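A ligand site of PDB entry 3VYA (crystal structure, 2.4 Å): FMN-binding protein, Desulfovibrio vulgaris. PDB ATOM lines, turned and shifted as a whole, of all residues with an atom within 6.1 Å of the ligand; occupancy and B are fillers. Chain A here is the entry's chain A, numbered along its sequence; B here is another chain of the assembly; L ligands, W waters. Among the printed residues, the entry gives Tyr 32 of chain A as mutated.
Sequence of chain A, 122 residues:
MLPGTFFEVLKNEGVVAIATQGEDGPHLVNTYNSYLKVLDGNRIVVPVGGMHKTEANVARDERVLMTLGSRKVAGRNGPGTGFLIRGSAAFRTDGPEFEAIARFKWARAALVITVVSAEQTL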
ATOM      1  N   VAL A  15       5.886 -17.762  -3.590  1.00  0.00           N
ATOM      2  CA  VAL A  15       5.921 -16.736  -2.558  1.00  0.00           C
ATOM      3  C   VAL A  15       4.797 -15.720  -2.788  1.00  0.00           C
ATOM      4  O   VAL A  15       4.609 -15.218  -3.882  1.00  0.00           O
ATOM      5  CB  VAL A  15       7.307 -16.030  -2.508  1.00  0.00           C
ATOM      6  CG1 VAL A  15       7.288 -14.829  -1.590  1.00  0.00           C
ATOM      7  CG2 VAL A  15       8.395 -17.033  -2.094  1.00  0.00           C
ATOM      8  N   HIS A  27       3.859  -0.771   2.932  1.00  0.00           N
ATOM      9  CA  HIS A  27       4.747  -1.819   3.460  1.00  0.00           C
ATOM     10  C   HIS A  27       4.481  -3.140   2.749  1.00  0.00           C
ATOM     11  O   HIS A  27       3.391  -3.369   2.243  1.00  0.00           O
ATOM     12  CB  HIS A  27       4.625  -1.962   4.986  1.00  0.00           C
ATOM     13  CG  HIS A  27       5.669  -2.851   5.592  1.00  0.00           C
ATOM     14  ND1 HIS A  27       7.016  -2.691   5.343  1.00  0.00           N
ATOM     15  CD2 HIS A  27       5.565  -3.889   6.449  1.00  0.00           C
ATOM     16  CE1 HIS A  27       7.691  -3.604   6.024  1.00  0.00           C
ATOM     17  NE2 HIS A  27       6.832  -4.349   6.698  1.00  0.00           N
ATOM     18  N   LEU A  28       5.498  -4.004   2.719  1.00  0.00           N
ATOM     19  CA  LEU A  28       5.469  -5.208   1.909  1.00  0.00           C
ATOM     20  C   LEU A  28       6.095  -6.384   2.650  1.00  0.00           C
ATOM     21  O   LEU A  28       7.249  -6.306   3.077  1.00  0.00           O
ATOM     22  CB  LEU A  28       6.211  -4.947   0.587  1.00  0.00           C
ATOM     23  CG  LEU A  28       6.011  -5.928  -0.571  1.00  0.00           C
ATOM     24  CD1 LEU A  28       4.555  -6.030  -0.961  1.00  0.00           C
ATOM     25  CD2 LEU A  28       6.855  -5.510  -1.768  1.00  0.00           C
ATOM     26  N   VAL A  29       5.315  -7.457   2.800  1.00  0.00           N
ATOM     27  CA  VAL A  29       5.761  -8.679   3.475  1.00  0.00           C
ATOM     28  C   VAL A  29       5.396  -9.939   2.677  1.00  0.00           C
ATOM     29  O   VAL A  29       4.610  -9.861   1.721  1.00  0.00           O
ATOM     30  CB  VAL A  29       5.230  -8.786   4.930  1.00  0.00           C
ATOM     31  CG1 VAL A  29       5.701  -7.615   5.787  1.00  0.00           C
ATOM     32  CG2 VAL A  29       3.698  -8.920   4.956  1.00  0.00           C
ATOM     33  N   ASN A  30       5.961 -11.082   3.069  1.00  0.00           N
ATOM     34  CA  ASN A  30       5.758 -12.335   2.338  1.00  0.00           C
ATOM     35  C   ASN A  30       5.189 -13.478   3.144  1.00  0.00           C
ATOM     36  O   ASN A  30       5.173 -13.434   4.365  1.00  0.00           O
ATOM     37  CB  ASN A  30       7.067 -12.826   1.699  1.00  0.00           C
ATOM     38  CG  ASN A  30       7.681 -11.810   0.781  1.00  0.00           C
ATOM     39  OD1 ASN A  30       8.715 -11.217   1.099  1.00  0.00           O
ATOM     40  ND2 ASN A  30       7.059 -11.589  -0.362  1.00  0.00           N
ATOM     41  N   THR A  31       4.731 -14.496   2.431  1.00  0.00           N
ATOM     42  CA  THR A  31       4.406 -15.822   2.974  1.00  0.00           C
ATOM     43  C   THR A  31       4.433 -16.799   1.803  1.00  0.00           C
ATOM     44  O   THR A  31       4.769 -16.420   0.702  1.00  0.00           O
ATOM     45  CB  THR A  31       3.047 -15.847   3.739  1.00  0.00           C
ATOM     46  OG1 THR A  31       2.851 -17.156   4.304  1.00  0.00           O
ATOM     47  CG2 THR A  31       1.877 -15.481   2.840  1.00  0.00           C
ATOM     48  N   TYR A  32       4.120 -18.068   2.037  1.00  0.00           N
ATOM     49  CA  TYR A  32       4.131 -19.044   0.941  1.00  0.00           C
ATOM     50  C   TYR A  32       2.726 -19.390   0.542  1.00  0.00           C
ATOM     51  O   TYR A  32       1.838 -19.427   1.389  1.00  0.00           O
ATOM     52  CB  TYR A  32       4.905 -20.302   1.321  1.00  0.00           C
ATOM     53  CG  TYR A  32       6.366 -20.071   1.568  1.00  0.00           C
ATOM     54  CD1 TYR A  32       7.272 -20.055   0.506  1.00  0.00           C
ATOM     55  CD2 TYR A  32       6.844 -19.841   2.848  1.00  0.00           C
ATOM     56  CE1 TYR A  32       8.631 -19.826   0.732  1.00  0.00           C
ATOM     57  CE2 TYR A  32       8.189 -19.602   3.089  1.00  0.00           C
ATOM     58  CZ  TYR A  32       9.075 -19.594   2.027  1.00  0.00           C
ATOM     59  OH  TYR A  32      10.408 -19.373   2.275  1.00  0.00           O
ATOM     60  N   TYR A  35       1.141 -21.959   2.638  1.00  0.00           N
ATOM     61  CA  TYR A  35       0.875 -21.588   4.026  1.00  0.00           C
ATOM     62  C   TYR A  35      -0.534 -21.017   4.165  1.00  0.00           C
ATOM     63  O   TYR A  35      -1.097 -21.032   5.253  1.00  0.00           O
ATOM     64  CB  TYR A  35       1.880 -20.540   4.500  1.00  0.00           C
ATOM     65  CG  TYR A  35       3.245 -21.038   4.937  1.00  0.00           C
ATOM     66  CD1 TYR A  35       3.783 -22.232   4.443  1.00  0.00           C
ATOM     67  CD2 TYR A  35       4.014 -20.296   5.823  1.00  0.00           C
ATOM     68  CE1 TYR A  35       5.054 -22.668   4.844  1.00  0.00           C
ATOM     69  CE2 TYR A  35       5.270 -20.720   6.229  1.00  0.00           C
ATOM     70  CZ  TYR A  35       5.784 -21.893   5.733  1.00  0.00           C
ATOM     71  OH  TYR A  35       7.024 -22.290   6.148  1.00  0.00           O
ATOM     72  N   VAL A  46      -3.617 -16.163   6.855  1.00  0.00           N
ATOM     73  CA  VAL A  46      -2.151 -16.181   6.806  1.00  0.00           C
ATOM     74  C   VAL A  46      -1.595 -16.377   8.213  1.00  0.00           C
ATOM     75  O   VAL A  46      -2.038 -15.733   9.152  1.00  0.00           O
ATOM     76  CB  VAL A  46      -1.604 -14.829   6.224  1.00  0.00           C
ATOM     77  CG1 VAL A  46      -0.117 -14.931   5.921  1.00  0.00           C
ATOM     78  CG2 VAL A  46      -2.365 -14.438   4.965  1.00  0.00           C
ATOM     79  N   PRO A  47      -0.615 -17.281   8.374  1.00  0.00           N
ATOM     80  CA  PRO A  47      -0.014 -17.421   9.697  1.00  0.00           C
ATOM     81  C   PRO A  47       0.909 -16.245  10.007  1.00  0.00           C
ATOM     82  O   PRO A  47       1.722 -15.860   9.158  1.00  0.00           O
ATOM     83  CB  PRO A  47       0.760 -18.730   9.595  1.00  0.00           C
ATOM     84  CG  PRO A  47       1.083 -18.855   8.131  1.00  0.00           C
ATOM     85  CD  PRO A  47      -0.072 -18.263   7.406  1.00  0.00           C
ATOM     86  N   VAL A  48       0.779 -15.680  11.203  1.00  0.00           N
ATOM     87  CA  VAL A  48       1.554 -14.509  11.600  1.00  0.00           C
ATOM     88  C   VAL A  48       2.629 -14.904  12.606  1.00  0.00           C
ATOM     89  O   VAL A  48       2.329 -15.392  13.684  1.00  0.00           O
ATOM     90  CB  VAL A  48       0.633 -13.410  12.183  1.00  0.00           C
ATOM     91  CG1 VAL A  48       1.443 -12.247  12.751  1.00  0.00           C
ATOM     92  CG2 VAL A  48      -0.364 -12.913  11.123  1.00  0.00           C
ATOM     93  N   GLY A  49       3.892 -14.728  12.225  1.00  0.00           N
ATOM     94  CA  GLY A  49       5.004 -14.922  13.124  1.00  0.00           C
ATOM     95  C   GLY A  49       5.521 -13.569  13.546  1.00  0.00           C
ATOM     96  O   GLY A  49       5.623 -13.274  14.739  1.00  0.00           O
ATOM     97  N   GLY A  50       5.841 -12.741  12.568  1.00  0.00           N
ATOM     98  CA  GLY A  50       6.328 -11.384  12.807  1.00  0.00           C
ATOM     99  C   GLY A  50       5.226 -10.383  12.477  1.00  0.00           C
ATOM    100  O   GLY A  50       4.312 -10.174  13.277  1.00  0.00           O
ATOM    101  N   MET A  51       5.314  -9.798  11.281  1.00  0.00           N
ATOM    102  CA  MET A  51       4.289  -8.875  10.776  1.00  0.00           C
ATOM    103  C   MET A  51       3.854  -7.838  11.810  1.00  0.00           C
ATOM    104  O   MET A  51       2.664  -7.588  11.996  1.00  0.00           O
ATOM    105  CB  MET A  51       3.083  -9.632  10.183  1.00  0.00           C
ATOM    106  CG  MET A  51       3.458 -10.524   9.007  1.00  0.00           C
ATOM    107  SD  MET A  51       2.053 -11.151   8.054  1.00  0.00           S
ATOM    108  CE  MET A  51       2.920 -12.197   6.888  1.00  0.00           C
ATOM    109  N   HIS A  52       4.830  -7.240  12.468  1.00  0.00           N
ATOM    110  CA  HIS A  52       4.581  -6.195  13.442  1.00  0.00           C
ATOM    111  C   HIS A  52       4.269  -4.854  12.795  1.00  0.00           C
ATOM    112  O   HIS A  52       3.322  -4.172  13.206  1.00  0.00           O
ATOM    113  CB  HIS A  52       5.757  -6.082  14.417  1.00  0.00           C
ATOM    114  CG  HIS A  52       6.068  -7.363  15.112  1.00  0.00           C
ATOM    115  ND1 HIS A  52       5.244  -7.906  16.076  1.00  0.00           N
ATOM    116  CD2 HIS A  52       7.089  -8.235  14.955  1.00  0.00           C
ATOM    117  CE1 HIS A  52       5.761  -9.051  16.493  1.00  0.00           C
ATOM    118  NE2 HIS A  52       6.880  -9.275  15.822  1.00  0.00           N
ATOM    119  N   LYS A  53       5.060  -4.462  11.784  1.00  0.00           N
ATOM    120  CA  LYS A  53       4.814  -3.207  11.065  1.00  0.00           C
ATOM    121  C   LYS A  53       3.508  -3.337  10.307  1.00  0.00           C
ATOM    122  O   LYS A  53       2.705  -2.392  10.253  1.00  0.00           O
ATOM    123  CB  LYS A  53       5.952  -2.888  10.111  1.00  0.00           C
ATOM    124  CG  LYS A  53       5.947  -1.484   9.552  1.00  0.00           C
ATOM    125  CD  LYS A  53       7.134  -1.304   8.607  1.00  0.00           C
ATOM    126  CE  LYS A  53       7.437   0.174   8.305  1.00  0.00           C
ATOM    127  NZ  LYS A  53       6.394   0.833   7.471  1.00  0.00           N
ATOM    128  N   THR A  54       3.291  -4.524   9.731  1.00  0.00           N
ATOM    129  CA  THR A  54       2.079  -4.819   8.982  1.00  0.00           C
ATOM    130  C   THR A  54       0.842  -4.662   9.866  1.00  0.00           C
ATOM    131  O   THR A  54      -0.153  -4.063   9.448  1.00  0.00           O
ATOM    132  CB  THR A  54       2.147  -6.220   8.348  1.00  0.00           C
ATOM    133  OG1 THR A  54       3.241  -6.256   7.418  1.00  0.00           O
ATOM    134  CG2 THR A  54       0.870  -6.567   7.613  1.00  0.00           C
ATOM    135  N   GLU A  55       0.900  -5.192  11.081  1.00  0.00           N
ATOM    136  CA  GLU A  55      -0.214  -5.087  12.022  1.00  0.00           C
ATOM    137  C   GLU A  55      -0.478  -3.631  12.410  1.00  0.00           C
ATOM    138  O   GLU A  55      -1.640  -3.231  12.508  1.00  0.00           O
ATOM    139  CB  GLU A  55       0.041  -5.955  13.260  1.00  0.00           C
ATOM    140  CG  GLU A  55      -1.106  -5.990  14.249  1.00  0.00           C
ATOM    141  CD  GLU A  55      -0.825  -6.840  15.480  1.00  0.00           C
ATOM    142  OE1 GLU A  55       0.317  -7.324  15.652  1.00  0.00           O
ATOM    143  OE2 GLU A  55      -1.759  -7.007  16.306  1.00  0.00           O
ATOM    144  N   TRP A 106       4.613 -21.560  15.663  1.00  0.00           N
ATOM    145  CA  TRP A 106       5.232 -20.250  15.812  1.00  0.00           C
ATOM    146  C   TRP A 106       4.272 -19.059  15.601  1.00  0.00           C
ATOM    147  O   TRP A 106       4.639 -17.913  15.880  1.00  0.00           O
ATOM    148  CB  TRP A 106       6.469 -20.120  14.901  1.00  0.00           C
ATOM    149  CG  TRP A 106       6.235 -20.523  13.454  1.00  0.00           C
ATOM    150  CD1 TRP A 106       6.593 -21.702  12.860  1.00  0.00           C
ATOM    151  CD2 TRP A 106       5.593 -19.741  12.433  1.00  0.00           C
ATOM    152  NE1 TRP A 106       6.218 -21.707  11.535  1.00  0.00           N
ATOM    153  CE2 TRP A 106       5.607 -20.515  11.245  1.00  0.00           C
ATOM    154  CE3 TRP A 106       5.018 -18.463  12.401  1.00  0.00           C
ATOM    155  CZ2 TRP A 106       5.052 -20.059  10.043  1.00  0.00           C
ATOM    156  CZ3 TRP A 106       4.483 -17.999  11.199  1.00  0.00           C
ATOM    157  CH2 TRP A 106       4.502 -18.797  10.046  1.00  0.00           C
ATOM    158  N   LEU B  68      12.030  -9.953  -3.033  1.00  0.00           N
ATOM    159  CA  LEU B  68      12.504 -11.015  -3.891  1.00  0.00           C
ATOM    160  C   LEU B  68      13.312 -11.948  -3.000  1.00  0.00           C
ATOM    161  O   LEU B  68      13.829 -11.519  -1.973  1.00  0.00           O
ATOM    162  CB  LEU B  68      13.377 -10.459  -5.023  1.00  0.00           C
ATOM    163  CG  LEU B  68      14.857 -10.173  -4.732  1.00  0.00           C
ATOM    164  CD1 LEU B  68      15.677 -10.040  -6.024  1.00  0.00           C
ATOM    165  CD2 LEU B  68      15.000  -8.928  -3.882  1.00  0.00           C
ATOM    166  N   GLY B  69      13.400 -13.203  -3.409  1.00  0.00           N
ATOM    167  CA  GLY B  69      14.191 -14.184  -2.697  1.00  0.00           C
ATOM    168  C   GLY B  69      14.230 -15.517  -3.423  1.00  0.00           C
ATOM    169  O   GLY B  69      13.809 -15.633  -4.575  1.00  0.00           O
ATOM    170  N   THR B  81      16.182 -17.551   1.659  1.00  0.00           N
ATOM    171  CA  THR B  81      16.475 -16.148   1.921  1.00  0.00           C
ATOM    172  C   THR B  81      15.542 -15.244   1.130  1.00  0.00           C
ATOM    173  O   THR B  81      15.188 -15.540  -0.014  1.00  0.00           O
ATOM    174  CB  THR B  81      17.971 -15.766   1.653  1.00  0.00           C
ATOM    175  OG1 THR B  81      18.284 -14.567   2.368  1.00  0.00           O
ATOM    176  CG2 THR B  81      18.249 -15.567   0.177  1.00  0.00           C
ATOM    177  N   GLY B  82      15.128 -14.160   1.789  1.00  0.00           N
ATOM    178  CA  GLY B  82      14.293 -13.146   1.184  1.00  0.00           C
ATOM    179  C   GLY B  82      14.838 -11.779   1.533  1.00  0.00           C
ATOM    180  O   GLY B  82      15.451 -11.587   2.591  1.00  0.00           O
ATOM    181  N   PHE B  83      14.647 -10.834   0.621  1.00  0.00           N
ATOM    182  CA  PHE B  83      15.060  -9.462   0.840  1.00  0.00           C
ATOM    183  C   PHE B  83      13.884  -8.522   0.763  1.00  0.00           C
ATOM    184  O   PHE B  83      12.926  -8.785   0.015  1.00  0.00           O
ATOM    185  CB  PHE B  83      16.104  -9.058  -0.205  1.00  0.00           C
ATOM    186  CG  PHE B  83      17.408  -9.821  -0.104  1.00  0.00           C
ATOM    187  CD1 PHE B  83      17.610 -10.987  -0.835  1.00  0.00           C
ATOM    188  CD2 PHE B  83      18.444  -9.343   0.714  1.00  0.00           C
ATOM    189  CE1 PHE B  83      18.806 -11.677  -0.754  1.00  0.00           C
ATOM    190  CE2 PHE B  83      19.663 -10.041   0.800  1.00  0.00           C
ATOM    191  CZ  PHE B  83      19.837 -11.210   0.072  1.00  0.00           C
ATOM    192  N   LEU B  84      13.944  -7.447   1.544  1.00  0.00           N
ATOM    193  CA  LEU B  84      13.074  -6.286   1.357  1.00  0.00           C
ATOM    194  C   LEU B  84      13.928  -5.086   0.952  1.00  0.00           C
ATOM    195  O   LEU B  84      14.805  -4.657   1.690  1.00  0.00           O
ATOM    196  CB  LEU B  84      12.243  -5.957   2.598  1.00  0.00           C
ATOM    197  CG  LEU B  84      11.445  -4.645   2.495  1.00  0.00           C
ATOM    198  CD1 LEU B  84      10.320  -4.740   1.467  1.00  0.00           C
ATOM    199  CD2 LEU B  84      10.910  -4.193   3.840  1.00  0.00           C
ATOM    200  N   THR B 121      14.949 -10.617   5.050  1.00  0.00           N
ATOM    201  CA  THR B 121      13.742 -10.898   5.824  1.00  0.00           C
ATOM    202  C   THR B 121      13.590 -12.387   6.118  1.00  0.00           C
ATOM    203  O   THR B 121      12.738 -12.794   6.902  1.00  0.00           O
ATOM    204  CB  THR B 121      12.486 -10.344   5.130  1.00  0.00           C
ATOM    205  OG1 THR B 121      12.467 -10.762   3.761  1.00  0.00           O
ATOM    206  CG2 THR B 121      12.486  -8.820   5.175  1.00  0.00           C
ATOM    207  N   LEU B 122      14.437 -13.198   5.485  1.00  0.00           N
ATOM    208  CA  LEU B 122      14.444 -14.637   5.691  1.00  0.00           C
ATOM    209  C   LEU B 122      15.879 -15.168   5.653  1.00  0.00           C
ATOM    210  O   LEU B 122      16.719 -14.733   4.846  1.00  0.00           O
ATOM    211  CB  LEU B 122      13.574 -15.345   4.659  1.00  0.00           C
ATOM    212  CG  LEU B 122      13.354 -16.867   4.794  1.00  0.00           C
ATOM    213  CD1 LEU B 122      12.161 -17.168   5.696  1.00  0.00           C
ATOM    214  CD2 LEU B 122      13.178 -17.522   3.419  1.00  0.00           C
ATOM    215  OXT LEU B 122      16.239 -16.051   6.439  1.00  0.00           O
HETATM  216  N1  LIG L   1       6.452 -13.819   8.235  1.00  0.00           N
HETATM  217  C1  LIG L   1       5.302 -14.300   8.866  1.00  0.00           C
HETATM  218  O1  LIG L   1       4.901 -13.733   9.884  1.00  0.00           O
HETATM  219  N2  LIG L   1       4.619 -15.407   8.341  1.00  0.00           N
HETATM  220  C2  LIG L   1       5.099 -16.033   7.184  1.00  0.00           C
HETATM  221  O2  LIG L   1       4.515 -17.009   6.714  1.00  0.00           O
HETATM  222  C3  LIG L   1       6.248 -15.538   6.557  1.00  0.00           C
HETATM  223  N3  LIG L   1       6.729 -16.153   5.413  1.00  0.00           N
HETATM  224  C4  LIG L   1       7.787 -15.604   4.696  1.00  0.00           C
HETATM  225  C5  LIG L   1       8.142 -16.162   3.477  1.00  0.00           C
HETATM  226  C6  LIG L   1       9.187 -15.638   2.744  1.00  0.00           C
HETATM  227  C7  LIG L   1       9.549 -16.304   1.412  1.00  0.00           C
HETATM  228  C8  LIG L   1       9.881 -14.533   3.226  1.00  0.00           C
HETATM  229  C9  LIG L   1      11.034 -13.930   2.420  1.00  0.00           C
HETATM  230  C10 LIG L   1       9.524 -13.958   4.439  1.00  0.00           C
HETATM  231  C11 LIG L   1       8.475 -14.495   5.190  1.00  0.00           C
HETATM  232  N4  LIG L   1       8.064 -13.930   6.427  1.00  0.00           N
HETATM  233  C12 LIG L   1       6.924 -14.436   7.071  1.00  0.00           C
HETATM  234  C13 LIG L   1       8.708 -12.706   6.946  1.00  0.00           C
HETATM  235  C14 LIG L   1       7.823 -11.474   6.655  1.00  0.00           C
HETATM  236  O3  LIG L   1       7.920 -11.159   5.272  1.00  0.00           O
HETATM  237  C15 LIG L   1       8.212 -10.237   7.465  1.00  0.00           C
HETATM  238  O4  LIG L   1       9.540  -9.814   7.112  1.00  0.00           O
HETATM  239  C16 LIG L   1       8.102 -10.432   8.997  1.00  0.00           C
HETATM  240  O5  LIG L   1       6.929 -11.175   9.320  1.00  0.00           O
HETATM  241  C17 LIG L   1       8.074  -9.082   9.717  1.00  0.00           C
HETATM  242  O6  LIG L   1       6.895  -8.370   9.349  1.00  0.00           O
HETATM  243  P1  LIG L   1       6.802  -6.730   9.351  1.00  0.00           P
HETATM  244  O7  LIG L   1       7.962  -6.199   8.379  1.00  0.00           O
HETATM  245  O8  LIG L   1       7.199  -6.286  10.823  1.00  0.00           O
HETATM  246  O9  LIG L   1       5.472  -6.211   8.927  1.00  0.00           O
HETATM  247  O   HOH W   1       9.712 -10.159   3.347  1.00  0.00           O
HETATM  248  O   HOH W   2       8.982  -6.287  12.628  1.00  0.00           O
HETATM  249  O   HOH W   3      11.565 -10.888   8.843  1.00  0.00           O
HETATM  250  O   HOH W   4       9.704  -7.169   6.680  1.00  0.00           O
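The backbone NH of Thr 54 sits at hydrogen-bond distance from an oxygen (O9) of the ligand (2.9 Å). An oxygen (O9) of the ligand is in hydrogen-bond range of the side-chain hydroxyl (OG1) of Thr 54, at 2.7 Å. N of Gly 49 sits at hydrogen-bond distance from O1 of the ligand, 2.7 Å away. A ring nitrogen (NE2) of His 27 sits at hydrogen-bond distance from an oxygen (O7) of the ligand. The backbone NH of Met 51 lies within hydrogen-bond range of an oxygen (O6) of the ligand (2.9 Å). OG1 of Thr 31 is in hydrogen-bond range of O2 of the ligand (2.9 Å). The backbone NH of Asn 30 is in hydrogen-bond range of an oxygen (O3) of the ligand, at 2.9 Å. N of Lys 53 lies within hydrogen-bond range of O8 of the ligand (3.0 Å). The backbone NH (N) of Gly 50 lies within hydrogen-bond range of an oxygen (O1) of the ligand (3.0 Å). The backbone NH of His 52 lies within hydrogen-bond range of an oxygen (O8) of the ligand (3.0 Å). A nitrogen (N2) of the ligand lies within hydrogen-bond range of the backbone carbonyl oxygen (O) of Pro 47, at 3.0 Å.
The backbone carbonyl oxygen of Gly 82 of chain B is in hydrogen-bond range of the backbone NH of Thr 121 of chain B (2.7 Å). The backbone carbonyl oxygen (O) of Gly 82 of chain B sits at hydrogen-bond distance from the backbone NH (N) of Leu 122 of chain B (3.5 Å). The side-chain hydroxyl (OG1) of Thr 81 of chain B is in hydrogen-bond range of the chain-end carboxylate (O) of Leu 122 of chain B (2.9 Å).
Residues that only touch the ligand: Val 15, Val 29, Tyr 32, Tyr 35, Val 48, Trp 106, Gly 82 of chain B, Thr 121 of chain B and Leu 122 of chain B. Within 4 Å of the ligand: Val 15, His 27, Val 29, Asn 30, Thr 31, Tyr 32, Tyr 35, Pro 47, Val 48, Gly 49, Gly 50, Met 51, His 52, Lys 53, Thr 54, Trp 106, Gly 82 of chain B, Thr 121 of chain B and Leu 122 of chain B.
Water W1 lies within hydrogen-bond range of the side-chain amide oxygen (OD1) of Asn 30 (2.7 Å), an oxygen (O3) of the ligand (2.8 Å) and the side-chain hydroxyl (OG1) of Thr 121 of chain B (2.9 Å). Water W3 bridges O4 of the ligand (2.9 Å) and O of Thr 121 of chain B (3.0 Å).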
